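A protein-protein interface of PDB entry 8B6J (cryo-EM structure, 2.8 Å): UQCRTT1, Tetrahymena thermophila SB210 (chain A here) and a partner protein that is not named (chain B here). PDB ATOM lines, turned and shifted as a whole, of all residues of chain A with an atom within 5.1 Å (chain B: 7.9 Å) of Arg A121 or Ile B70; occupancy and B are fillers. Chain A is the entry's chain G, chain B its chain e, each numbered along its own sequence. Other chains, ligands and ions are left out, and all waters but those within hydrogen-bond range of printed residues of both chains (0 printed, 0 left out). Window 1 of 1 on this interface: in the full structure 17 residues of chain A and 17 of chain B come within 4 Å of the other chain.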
ATOM      1  N   LYS A 117      18.780 -14.867 -24.749  1.00  0.00           N
ATOM      2  CA  LYS A 117      19.570 -15.856 -24.024  1.00  0.00           C
ATOM      3  C   LYS A 117      19.688 -17.165 -24.792  1.00  0.00           C
ATOM      4  O   LYS A 117      20.707 -17.856 -24.681  1.00  0.00           O
ATOM      5  CB  LYS A 117      18.960 -16.107 -22.645  1.00  0.00           C
ATOM      6  CG  LYS A 117      19.103 -14.942 -21.679  1.00  0.00           C
ATOM      7  CD  LYS A 117      20.559 -14.682 -21.324  1.00  0.00           C
ATOM      8  CE  LYS A 117      20.693 -13.577 -20.293  1.00  0.00           C
ATOM      9  NZ  LYS A 117      22.115 -13.315 -19.945  1.00  0.00           N
ATOM     10  N   ARG A 118      18.666 -17.528 -25.568  1.00  0.00           N
ATOM     11  CA  ARG A 118      18.754 -18.749 -26.361  1.00  0.00           C
ATOM     12  C   ARG A 118      19.911 -18.674 -27.349  1.00  0.00           C
ATOM     13  O   ARG A 118      20.631 -19.659 -27.548  1.00  0.00           O
ATOM     14  CB  ARG A 118      17.437 -18.995 -27.091  1.00  0.00           C
ATOM     15  CG  ARG A 118      16.393 -19.720 -26.259  1.00  0.00           C
ATOM     16  CD  ARG A 118      15.076 -19.810 -27.001  1.00  0.00           C
ATOM     17  NE  ARG A 118      14.242 -18.636 -26.780  1.00  0.00           N
ATOM     18  CZ  ARG A 118      13.256 -18.252 -27.578  1.00  0.00           C
ATOM     19  NH1 ARG A 118      12.975 -18.905 -28.694  1.00  0.00           N
ATOM     20  NH2 ARG A 118      12.536 -17.182 -27.253  1.00  0.00           N
ATOM     21  N   ARG A 119      20.103 -17.515 -27.981  1.00  0.00           N
ATOM     22  CA  ARG A 119      21.249 -17.346 -28.866  1.00  0.00           C
ATOM     23  C   ARG A 119      22.544 -17.186 -28.082  1.00  0.00           C
ATOM     24  O   ARG A 119      23.606 -17.616 -28.551  1.00  0.00           O
ATOM     25  CB  ARG A 119      21.037 -16.140 -29.780  1.00  0.00           C
ATOM     26  CG  ARG A 119      20.035 -16.379 -30.893  1.00  0.00           C
ATOM     27  CD  ARG A 119      20.149 -15.321 -31.971  1.00  0.00           C
ATOM     28  NE  ARG A 119      19.412 -15.677 -33.176  1.00  0.00           N
ATOM     29  CZ  ARG A 119      18.125 -15.424 -33.374  1.00  0.00           C
ATOM     30  NH1 ARG A 119      17.387 -14.822 -32.456  1.00  0.00           N
ATOM     31  NH2 ARG A 119      17.563 -15.789 -34.523  1.00  0.00           N
ATOM     32  N   ALA A 120      22.482 -16.563 -26.902  1.00  0.00           N
ATOM     33  CA  ALA A 120      23.685 -16.395 -26.093  1.00  0.00           C
ATOM     34  C   ALA A 120      24.276 -17.743 -25.709  1.00  0.00           C
ATOM     35  O   ALA A 120      25.499 -17.929 -25.755  1.00  0.00           O
ATOM     36  CB  ALA A 120      23.367 -15.572 -24.846  1.00  0.00           C
ATOM     37  N   ARG A 121      23.421 -18.695 -25.323  1.00  0.00           N
ATOM     38  CA  ARG A 121      23.871 -20.055 -25.045  1.00  0.00           C
ATOM     39  C   ARG A 121      24.864 -20.522 -26.097  1.00  0.00           C
ATOM     40  O   ARG A 121      26.026 -20.823 -25.803  1.00  0.00           O
ATOM     41  CB  ARG A 121      22.688 -21.026 -25.044  1.00  0.00           C
ATOM     42  CG  ARG A 121      21.678 -20.922 -23.933  1.00  0.00           C
ATOM     43  CD  ARG A 121      20.589 -21.948 -24.216  1.00  0.00           C
ATOM     44  NE  ARG A 121      19.560 -22.029 -23.191  1.00  0.00           N
ATOM     45  CZ  ARG A 121      18.513 -22.841 -23.257  1.00  0.00           C
ATOM     46  NH1 ARG A 121      18.329 -23.649 -24.288  1.00  0.00           N
ATOM     47  NH2 ARG A 121      17.629 -22.841 -22.265  1.00  0.00           N
ATOM     48  N   TYR A 122      24.394 -20.582 -27.343  1.00  0.00           N
ATOM     49  CA  TYR A 122      25.196 -21.137 -28.425  1.00  0.00           C
ATOM     50  C   TYR A 122      26.398 -20.258 -28.734  1.00  0.00           C
ATOM     51  O   TYR A 122      27.506 -20.767 -28.941  1.00  0.00           O
ATOM     52  CB  TYR A 122      24.324 -21.312 -29.668  1.00  0.00           C
ATOM     53  CG  TYR A 122      25.068 -21.794 -30.888  1.00  0.00           C
ATOM     54  CD1 TYR A 122      25.336 -23.141 -31.072  1.00  0.00           C
ATOM     55  CD2 TYR A 122      25.492 -20.904 -31.861  1.00  0.00           C
ATOM     56  CE1 TYR A 122      26.012 -23.587 -32.189  1.00  0.00           C
ATOM     57  CE2 TYR A 122      26.167 -21.339 -32.980  1.00  0.00           C
ATOM     58  CZ  TYR A 122      26.425 -22.682 -33.139  1.00  0.00           C
ATOM     59  OH  TYR A 122      27.099 -23.120 -34.255  1.00  0.00           O
ATOM     60  N   TYR A 123      26.212 -18.938 -28.769  1.00  0.00           N
ATOM     61  CA  TYR A 123      27.274 -18.083 -29.279  1.00  0.00           C
ATOM     62  C   TYR A 123      28.419 -17.912 -28.290  1.00  0.00           C
ATOM     63  O   TYR A 123      29.561 -17.709 -28.715  1.00  0.00           O
ATOM     64  CB  TYR A 123      26.704 -16.728 -29.693  1.00  0.00           C
ATOM     65  CG  TYR A 123      26.106 -16.771 -31.079  1.00  0.00           C
ATOM     66  CD1 TYR A 123      26.919 -16.796 -32.202  1.00  0.00           C
ATOM     67  CD2 TYR A 123      24.733 -16.808 -31.265  1.00  0.00           C
ATOM     68  CE1 TYR A 123      26.383 -16.845 -33.470  1.00  0.00           C
ATOM     69  CE2 TYR A 123      24.187 -16.856 -32.531  1.00  0.00           C
ATOM     70  CZ  TYR A 123      25.017 -16.875 -33.629  1.00  0.00           C
ATOM     71  OH  TYR A 123      24.476 -16.924 -34.892  1.00  0.00           O
ATOM     72  N   LYS A 124      28.156 -18.021 -26.984  1.00  0.00           N
ATOM     73  CA  LYS A 124      29.255 -18.004 -26.024  1.00  0.00           C
ATOM     74  C   LYS A 124      30.283 -19.075 -26.363  1.00  0.00           C
ATOM     75  O   LYS A 124      31.493 -18.853 -26.235  1.00  0.00           O
ATOM     76  CB  LYS A 124      28.722 -18.208 -24.606  1.00  0.00           C
ATOM     77  CG  LYS A 124      29.805 -18.202 -23.536  1.00  0.00           C
ATOM     78  CD  LYS A 124      29.229 -18.373 -22.143  1.00  0.00           C
ATOM     79  CE  LYS A 124      28.687 -19.774 -21.927  1.00  0.00           C
ATOM     80  NZ  LYS A 124      28.230 -19.979 -20.528  1.00  0.00           N
ATOM     81  N   VAL A 125      29.817 -20.245 -26.800  1.00  0.00           N
ATOM     82  CA  VAL A 125      30.723 -21.323 -27.178  1.00  0.00           C
ATOM     83  C   VAL A 125      31.216 -21.139 -28.607  1.00  0.00           C
ATOM     84  O   VAL A 125      32.384 -21.407 -28.911  1.00  0.00           O
ATOM     85  CB  VAL A 125      30.023 -22.681 -26.994  1.00  0.00           C
ATOM     86  CG1 VAL A 125      30.928 -23.810 -27.451  1.00  0.00           C
ATOM     87  CG2 VAL A 125      29.607 -22.874 -25.545  1.00  0.00           C
ATOM     88  N   PHE A 132      30.466 -25.244 -33.396  1.00  0.00           N
ATOM     89  CA  PHE A 132      29.755 -25.844 -32.277  1.00  0.00           C
ATOM     90  C   PHE A 132      28.461 -26.492 -32.751  1.00  0.00           C
ATOM     91  O   PHE A 132      27.684 -25.884 -33.494  1.00  0.00           O
ATOM     92  CB  PHE A 132      29.458 -24.784 -31.217  1.00  0.00           C
ATOM     93  CG  PHE A 132      28.766 -25.318 -29.993  1.00  0.00           C
ATOM     94  CD1 PHE A 132      28.982 -26.615 -29.559  1.00  0.00           C
ATOM     95  CD2 PHE A 132      27.892 -24.519 -29.277  1.00  0.00           C
ATOM     96  CE1 PHE A 132      28.345 -27.100 -28.437  1.00  0.00           C
ATOM     97  CE2 PHE A 132      27.252 -25.000 -28.154  1.00  0.00           C
ATOM     98  CZ  PHE A 132      27.479 -26.292 -27.734  1.00  0.00           C
ATOM     99  N   VAL A 134      25.042 -28.189 -31.130  1.00  0.00           N
ATOM    100  CA  VAL A 134      24.306 -28.249 -29.861  1.00  0.00           C
ATOM    101  C   VAL A 134      24.056 -29.706 -29.491  1.00  0.00           C
ATOM    102  O   VAL A 134      23.661 -30.502 -30.362  1.00  0.00           O
ATOM    103  CB  VAL A 134      22.994 -27.472 -29.978  1.00  0.00           C
ATOM    104  CG1 VAL A 134      22.037 -27.859 -28.873  1.00  0.00           C
ATOM    105  CG2 VAL A 134      23.271 -25.979 -29.939  1.00  0.00           C
ATOM    106  N   PRO A 135      24.266 -30.110 -28.229  1.00  0.00           N
ATOM    107  CA  PRO A 135      24.032 -31.512 -27.860  1.00  0.00           C
ATOM    108  C   PRO A 135      22.567 -31.907 -27.943  1.00  0.00           C
ATOM    109  O   PRO A 135      21.706 -31.073 -28.241  1.00  0.00           O
ATOM    110  CB  PRO A 135      24.556 -31.589 -26.420  1.00  0.00           C
ATOM    111  CG  PRO A 135      24.489 -30.198 -25.917  1.00  0.00           C
ATOM    112  CD  PRO A 135      24.785 -29.328 -27.094  1.00  0.00           C
ATOM    113  N   TRP A 137      20.379 -32.954 -25.607  1.00  0.00           N
ATOM    114  CA  TRP A 137      19.436 -32.544 -24.568  1.00  0.00           C
ATOM    115  C   TRP A 137      18.838 -31.174 -24.870  1.00  0.00           C
ATOM    116  O   TRP A 137      17.640 -30.955 -24.663  1.00  0.00           O
ATOM    117  CB  TRP A 137      20.110 -32.562 -23.193  1.00  0.00           C
ATOM    118  CG  TRP A 137      21.416 -31.827 -23.097  1.00  0.00           C
ATOM    119  CD1 TRP A 137      22.642 -32.278 -23.491  1.00  0.00           C
ATOM    120  CD2 TRP A 137      21.630 -30.523 -22.545  1.00  0.00           C
ATOM    121  NE1 TRP A 137      23.601 -31.332 -23.232  1.00  0.00           N
ATOM    122  CE2 TRP A 137      23.006 -30.245 -22.651  1.00  0.00           C
ATOM    123  CE3 TRP A 137      20.790 -29.561 -21.978  1.00  0.00           C
ATOM    124  CZ2 TRP A 137      23.561 -29.047 -22.211  1.00  0.00           C
ATOM    125  CZ3 TRP A 137      21.342 -28.372 -21.542  1.00  0.00           C
ATOM    126  CH2 TRP A 137      22.714 -28.125 -21.662  1.00  0.00           C
ATOM    127  N   VAL A 138      19.654 -30.238 -25.359  1.00  0.00           N
ATOM    128  CA  VAL A 138      19.122 -28.944 -25.778  1.00  0.00           C
ATOM    129  C   VAL A 138      18.299 -29.091 -27.052  1.00  0.00           C
ATOM    130  O   VAL A 138      17.249 -28.453 -27.212  1.00  0.00           O
ATOM    131  CB  VAL A 138      20.269 -27.935 -25.965  1.00  0.00           C
ATOM    132  CG1 VAL A 138      19.752 -26.644 -26.583  1.00  0.00           C
ATOM    133  CG2 VAL A 138      20.952 -27.656 -24.642  1.00  0.00           C
ATOM    134  N   GLU A 141      14.533 -30.171 -26.435  1.00  0.00           N
ATOM    135  CA  GLU A 141      13.645 -29.093 -26.018  1.00  0.00           C
ATOM    136  C   GLU A 141      13.446 -28.080 -27.136  1.00  0.00           C
ATOM    137  O   GLU A 141      12.373 -27.476 -27.240  1.00  0.00           O
ATOM    138  CB  GLU A 141      14.191 -28.406 -24.765  1.00  0.00           C
ATOM    139  CG  GLU A 141      15.566 -27.787 -24.930  1.00  0.00           C
ATOM    140  CD  GLU A 141      15.991 -26.988 -23.714  1.00  0.00           C
ATOM    141  OE1 GLU A 141      15.302 -27.073 -22.676  1.00  0.00           O
ATOM    142  OE2 GLU A 141      17.012 -26.273 -23.797  1.00  0.00           O
ATOM    143  N   LEU B  43      33.703 -29.717 -25.884  1.00  0.00           N
ATOM    144  CA  LEU B  43      33.572 -30.219 -24.519  1.00  0.00           C
ATOM    145  C   LEU B  43      32.335 -29.586 -23.896  1.00  0.00           C
ATOM    146  O   LEU B  43      32.366 -28.437 -23.450  1.00  0.00           O
ATOM    147  CB  LEU B  43      34.824 -29.903 -23.713  1.00  0.00           C
ATOM    148  CG  LEU B  43      34.841 -30.385 -22.261  1.00  0.00           C
ATOM    149  CD1 LEU B  43      34.774 -31.902 -22.195  1.00  0.00           C
ATOM    150  CD2 LEU B  43      36.078 -29.870 -21.550  1.00  0.00           C
ATOM    151  N   VAL B  44      31.238 -30.343 -23.861  1.00  0.00           N
ATOM    152  CA  VAL B  44      29.959 -29.849 -23.373  1.00  0.00           C
ATOM    153  C   VAL B  44      29.408 -30.829 -22.348  1.00  0.00           C
ATOM    154  O   VAL B  44      29.811 -31.992 -22.282  1.00  0.00           O
ATOM    155  CB  VAL B  44      28.941 -29.644 -24.516  1.00  0.00           C
ATOM    156  CG1 VAL B  44      29.527 -28.749 -25.592  1.00  0.00           C
ATOM    157  CG2 VAL B  44      28.517 -30.983 -25.100  1.00  0.00           C
ATOM    158  N   GLU B  45      28.474 -30.337 -21.542  1.00  0.00           N
ATOM    159  CA  GLU B  45      27.810 -31.177 -20.559  1.00  0.00           C
ATOM    160  C   GLU B  45      26.906 -32.193 -21.247  1.00  0.00           C
ATOM    161  O   GLU B  45      26.325 -31.929 -22.303  1.00  0.00           O
ATOM    162  CB  GLU B  45      26.991 -30.318 -19.598  1.00  0.00           C
ATOM    163  CG  GLU B  45      27.813 -29.296 -18.835  1.00  0.00           C
ATOM    164  CD  GLU B  45      26.953 -28.241 -18.172  1.00  0.00           C
ATOM    165  OE1 GLU B  45      25.886 -27.906 -18.728  1.00  0.00           O
ATOM    166  OE2 GLU B  45      27.340 -27.749 -17.092  1.00  0.00           O
ATOM    167  N   ASP B  46      26.791 -33.369 -20.635  1.00  0.00           N
ATOM    168  CA  ASP B  46      25.948 -34.432 -21.162  1.00  0.00           C
ATOM    169  C   ASP B  46      24.500 -34.327 -20.705  1.00  0.00           C
ATOM    170  O   ASP B  46      23.665 -35.112 -21.165  1.00  0.00           O
ATOM    171  CB  ASP B  46      26.507 -35.798 -20.752  1.00  0.00           C
ATOM    172  CG  ASP B  46      27.872 -36.072 -21.350  1.00  0.00           C
ATOM    173  OD1 ASP B  46      28.361 -35.227 -22.130  1.00  0.00           O
ATOM    174  OD2 ASP B  46      28.456 -37.131 -21.042  1.00  0.00           O
ATOM    175  N   LYS B  47      24.184 -33.387 -19.822  1.00  0.00           N
ATOM    176  CA  LYS B  47      22.827 -33.206 -19.331  1.00  0.00           C
ATOM    177  C   LYS B  47      22.690 -31.780 -18.823  1.00  0.00           C
ATOM    178  O   LYS B  47      23.698 -31.114 -18.560  1.00  0.00           O
ATOM    179  CB  LYS B  47      22.498 -34.210 -18.214  1.00  0.00           C
ATOM    180  CG  LYS B  47      23.403 -34.095 -16.996  1.00  0.00           C
ATOM    181  CD  LYS B  47      23.078 -35.144 -15.941  1.00  0.00           C
ATOM    182  CE  LYS B  47      21.669 -34.983 -15.387  1.00  0.00           C
ATOM    183  NZ  LYS B  47      21.420 -33.613 -14.856  1.00  0.00           N
ATOM    184  N   PRO B  48      21.463 -31.279 -18.681  1.00  0.00           N
ATOM    185  CA  PRO B  48      21.287 -29.922 -18.150  1.00  0.00           C
ATOM    186  C   PRO B  48      21.921 -29.786 -16.774  1.00  0.00           C
ATOM    187  O   PRO B  48      21.828 -30.683 -15.933  1.00  0.00           O
ATOM    188  CB  PRO B  48      19.765 -29.757 -18.088  1.00  0.00           C
ATOM    189  CG  PRO B  48      19.223 -30.763 -19.038  1.00  0.00           C
ATOM    190  CD  PRO B  48      20.178 -31.911 -19.021  1.00  0.00           C
ATOM    191  N   THR B  49      22.569 -28.646 -16.548  1.00  0.00           N
ATOM    192  CA  THR B  49      23.197 -28.342 -15.271  1.00  0.00           C
ATOM    193  C   THR B  49      22.788 -26.947 -14.830  1.00  0.00           C
ATOM    194  O   THR B  49      22.679 -26.033 -15.653  1.00  0.00           O
ATOM    195  CB  THR B  49      24.725 -28.423 -15.352  1.00  0.00           C
ATOM    196  OG1 THR B  49      25.222 -27.330 -16.131  1.00  0.00           O
ATOM    197  CG2 THR B  49      25.158 -29.736 -15.983  1.00  0.00           C
ATOM    198  N   PHE B  50      22.562 -26.790 -13.529  1.00  0.00           N
ATOM    199  CA  PHE B  50      22.161 -25.517 -12.950  1.00  0.00           C
ATOM    200  C   PHE B  50      23.014 -25.241 -11.724  1.00  0.00           C
ATOM    201  O   PHE B  50      23.133 -26.096 -10.841  1.00  0.00           O
ATOM    202  CB  PHE B  50      20.678 -25.528 -12.575  1.00  0.00           C
ATOM    203  CG  PHE B  50      19.771 -25.914 -13.707  1.00  0.00           C
ATOM    204  CD1 PHE B  50      19.476 -27.242 -13.952  1.00  0.00           C
ATOM    205  CD2 PHE B  50      19.204 -24.947 -14.516  1.00  0.00           C
ATOM    206  CE1 PHE B  50      18.638 -27.600 -14.989  1.00  0.00           C
ATOM    207  CE2 PHE B  50      18.366 -25.300 -15.554  1.00  0.00           C
ATOM    208  CZ  PHE B  50      18.083 -26.627 -15.789  1.00  0.00           C
ATOM    209  N   ASP B  65      14.099 -22.587 -14.723  1.00  0.00           N
ATOM    210  CA  ASP B  65      14.293 -23.834 -15.456  1.00  0.00           C
ATOM    211  C   ASP B  65      15.085 -23.632 -16.741  1.00  0.00           C
ATOM    212  O   ASP B  65      15.630 -24.603 -17.278  1.00  0.00           O
ATOM    213  CB  ASP B  65      12.938 -24.466 -15.774  1.00  0.00           C
ATOM    214  CG  ASP B  65      13.064 -25.879 -16.304  1.00  0.00           C
ATOM    215  OD1 ASP B  65      14.179 -26.438 -16.260  1.00  0.00           O
ATOM    216  OD2 ASP B  65      12.045 -26.434 -16.763  1.00  0.00           O
ATOM    217  N   PHE B  66      15.158 -22.405 -17.245  1.00  0.00           N
ATOM    218  CA  PHE B  66      15.906 -22.133 -18.464  1.00  0.00           C
ATOM    219  C   PHE B  66      17.357 -22.573 -18.304  1.00  0.00           C
ATOM    220  O   PHE B  66      18.003 -22.272 -17.296  1.00  0.00           O
ATOM    221  CB  PHE B  66      15.830 -20.641 -18.787  1.00  0.00           C
ATOM    222  CG  PHE B  66      16.392 -20.274 -20.129  1.00  0.00           C
ATOM    223  CD1 PHE B  66      15.610 -20.359 -21.266  1.00  0.00           C
ATOM    224  CD2 PHE B  66      17.695 -19.830 -20.251  1.00  0.00           C
ATOM    225  CE1 PHE B  66      16.122 -20.017 -22.499  1.00  0.00           C
ATOM    226  CE2 PHE B  66      18.211 -19.488 -21.482  1.00  0.00           C
ATOM    227  CZ  PHE B  66      17.424 -19.581 -22.607  1.00  0.00           C
ATOM    228  N   LYS B  67      17.868 -23.293 -19.303  1.00  0.00           N
ATOM    229  CA  LYS B  67      19.248 -23.779 -19.294  1.00  0.00           C
ATOM    230  C   LYS B  67      20.133 -22.688 -19.879  1.00  0.00           C
ATOM    231  O   LYS B  67      20.362 -22.621 -21.087  1.00  0.00           O
ATOM    232  CB  LYS B  67      19.375 -25.079 -20.078  1.00  0.00           C
ATOM    233  CG  LYS B  67      18.598 -26.254 -19.498  1.00  0.00           C
ATOM    234  CD  LYS B  67      17.131 -26.211 -19.889  1.00  0.00           C
ATOM    235  CE  LYS B  67      16.427 -27.507 -19.539  1.00  0.00           C
ATOM    236  NZ  LYS B  67      15.003 -27.491 -19.963  1.00  0.00           N
ATOM    237  N   VAL B  68      20.645 -21.821 -19.006  1.00  0.00           N
ATOM    238  CA  VAL B  68      21.450 -20.695 -19.467  1.00  0.00           C
ATOM    239  C   VAL B  68      22.781 -21.177 -20.032  1.00  0.00           C
ATOM    240  O   VAL B  68      23.286 -20.628 -21.018  1.00  0.00           O
ATOM    241  CB  VAL B  68      21.654 -19.684 -18.324  1.00  0.00           C
ATOM    242  CG1 VAL B  68      20.315 -19.165 -17.830  1.00  0.00           C
ATOM    243  CG2 VAL B  68      22.439 -20.311 -17.183  1.00  0.00           C
ATOM    244  N   ASN B  69      23.371 -22.202 -19.423  1.00  0.00           N
ATOM    245  CA  ASN B  69      24.683 -22.705 -19.806  1.00  0.00           C
ATOM    246  C   ASN B  69      24.537 -24.024 -20.548  1.00  0.00           C
ATOM    247  O   ASN B  69      23.833 -24.927 -20.083  1.00  0.00           O
ATOM    248  CB  ASN B  69      25.573 -22.898 -18.577  1.00  0.00           C
ATOM    249  CG  ASN B  69      25.804 -21.614 -17.817  1.00  0.00           C
ATOM    250  OD1 ASN B  69      26.089 -20.573 -18.407  1.00  0.00           O
ATOM    251  ND2 ASN B  69      25.673 -21.675 -16.498  1.00  0.00           N
ATOM    252  N   ILE B  70      25.203 -24.132 -21.696  1.00  0.00           N
ATOM    253  CA  ILE B  70      25.279 -25.391 -22.428  1.00  0.00           C
ATOM    254  C   ILE B  70      26.614 -26.052 -22.117  1.00  0.00           C
ATOM    255  O   ILE B  70      26.740 -27.279 -22.187  1.00  0.00           O
ATOM    256  CB  ILE B  70      25.105 -25.177 -23.943  1.00  0.00           C
ATOM    257  CG1 ILE B  70      23.697 -24.661 -24.242  1.00  0.00           C
ATOM    258  CG2 ILE B  70      25.378 -26.478 -24.699  1.00  0.00           C
ATOM    259  CD1 ILE B  70      23.417 -24.439 -25.714  1.00  0.00           C
ATOM    260  N   ASP B  71      27.616 -25.248 -21.772  1.00  0.00           N
ATOM    261  CA  ASP B  71      28.959 -25.734 -21.499  1.00  0.00           C
ATOM    262  C   ASP B  71      29.412 -25.286 -20.117  1.00  0.00           C
ATOM    263  O   ASP B  71      29.022 -24.221 -19.631  1.00  0.00           O
ATOM    264  CB  ASP B  71      29.953 -25.238 -22.551  1.00  0.00           C
ATOM    265  CG  ASP B  71      29.694 -25.828 -23.921  1.00  0.00           C
ATOM    266  OD1 ASP B  71      28.653 -26.496 -24.090  1.00  0.00           O
ATOM    267  OD2 ASP B  71      30.531 -25.630 -24.825  1.00  0.00           O
ATOM    268  N   ASN B  72      30.245 -26.115 -19.494  1.00  0.00           N
ATOM    269  CA  ASN B  72      30.781 -25.860 -18.159  1.00  0.00           C
ATOM    270  C   ASN B  72      32.236 -25.413 -18.217  1.00  0.00           C
ATOM    271  O   ASN B  72      33.052 -25.801 -17.377  1.00  0.00           O
ATOM    272  CB  ASN B  72      30.635 -27.104 -17.288  1.00  0.00           C
ATOM    273  CG  ASN B  72      30.816 -26.809 -15.815  1.00  0.00           C
ATOM    274  OD1 ASN B  72      30.789 -25.653 -15.395  1.00  0.00           O
ATOM    275  ND2 ASN B  72      30.994 -27.856 -15.019  1.00  0.00           N
ATOM    276  N   TRP B  73      32.586 -24.592 -19.209  1.00  0.00           N
ATOM    277  CA  TRP B  73      33.970 -24.165 -19.375  1.00  0.00           C
ATOM    278  C   TRP B  73      34.497 -23.407 -18.165  1.00  0.00           C
ATOM    279  O   TRP B  73      35.716 -23.304 -18.000  1.00  0.00           O
ATOM    280  CB  TRP B  73      34.102 -23.283 -20.616  1.00  0.00           C
ATOM    281  CG  TRP B  73      33.963 -24.020 -21.909  1.00  0.00           C
ATOM    282  CD1 TRP B  73      33.647 -25.335 -22.076  1.00  0.00           C
ATOM    283  CD2 TRP B  73      34.138 -23.479 -23.222  1.00  0.00           C
ATOM    284  NE1 TRP B  73      33.614 -25.647 -23.411  1.00  0.00           N
ATOM    285  CE2 TRP B  73      33.912 -24.524 -24.136  1.00  0.00           C
ATOM    286  CE3 TRP B  73      34.464 -22.212 -23.713  1.00  0.00           C
ATOM    287  CZ2 TRP B  73      34.002 -24.342 -25.513  1.00  0.00           C
ATOM    288  CZ3 TRP B  73      34.552 -22.033 -25.078  1.00  0.00           C
ATOM    289  CH2 TRP B  73      34.322 -23.091 -25.964  1.00  0.00           C
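Hydrophobic or aromatic side chains of chain B that line the printed part of chain A: Val B44, Pro B48, Phe B66, Ile B70 and Trp B73. Along chain B the printed residues that touch a printed residue of chain A span positions 44 to 73. Of the 15 printed residues of chain A, 9 touch a printed residue of chain B. Hydrophobic or aromatic side chains of chain A within 4 Å of the printed part of chain B: Val A125, Phe A132, Pro A135 and Trp A137.
Arg A121 touches Phe B66. CG of Arg A121 touches O of Val B68, at 3.3 Å. Arg A121 touches Ile B70. CG2 of Val A125 touches OD2 of Asp B71, 3.0 Å away. CG1 of Val B44 touches CE1 of Phe A132, 3.5 Å away. CZ of Phe A132 touches OD1 of Asp B71, 3.8 Å away. Pro A135 touches Ile B70 (CD to CG2, 3.8 Å). Trp A137 touches Pro B48 (CE3 to CG, 3.5 Å). Trp A137 touches Asn B69. Ile B70 touches Trp A137 (O to CZ2, 3.6 Å).
NE1 of Trp A137 lies within hydrogen-bond range of O of Glu B45. The guanidinium group (NH2) of Arg A121 sits close to the backbone carbonyl oxygen (O) of Lys B67, 3.0 Å away. NZ of Lys B67 lies within salt-bridge range of OE1 of Glu A141 (2.8 Å). The side-chain amino group of Lys A124 sits at hydrogen-bond distance from the side-chain amide oxygen of Asn B69, 3.1 Å away.
NE1 of Trp B73 lies within hydrogen-bond range of O of Leu B43 (3.1 Å). OE1 of Glu B45 is in hydrogen-bond range of OG1 of Thr B49 (2.7 Å). OD1 of Asp B65 is in salt-bridge range of NZ of Lys B67, 3.9 Å away. The indole nitrogen (NE1) of Trp B73 sits at hydrogen-bond distance from the side-chain carboxylate (OD2) of Asp B71. The guanidinium group (NH1) of Arg A121 lies within salt-bridge range of the side-chain carboxylate (OE2) of Glu A141 (3.0 Å). The backbone carbonyl oxygen (O) of Phe A132 is in hydrogen-bond range of the side-chain hydroxyl (OH) of Tyr A122 (2.9 Å).
Ala A120 touches none of the printed residues of chain B. Arg A121 touches four residues of chain B. Tyr A122 touches none of the printed residues of chain B. Of the printed residues of chain B, Pro A135 touches Ile B70 (3.8 Å). Printed residues of chain B within 4 Å of Trp A137: Glu B45, Asp B46, Pro B48, Asn B69 and Ile B70. Of chain A, only Arg A121, Phe A132, Pro A135 and Trp A137 come within 4 Å of Ile B70. The nearest residue of chain B that does not touch Arg A121 is Asn B69 (5.0 Å).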
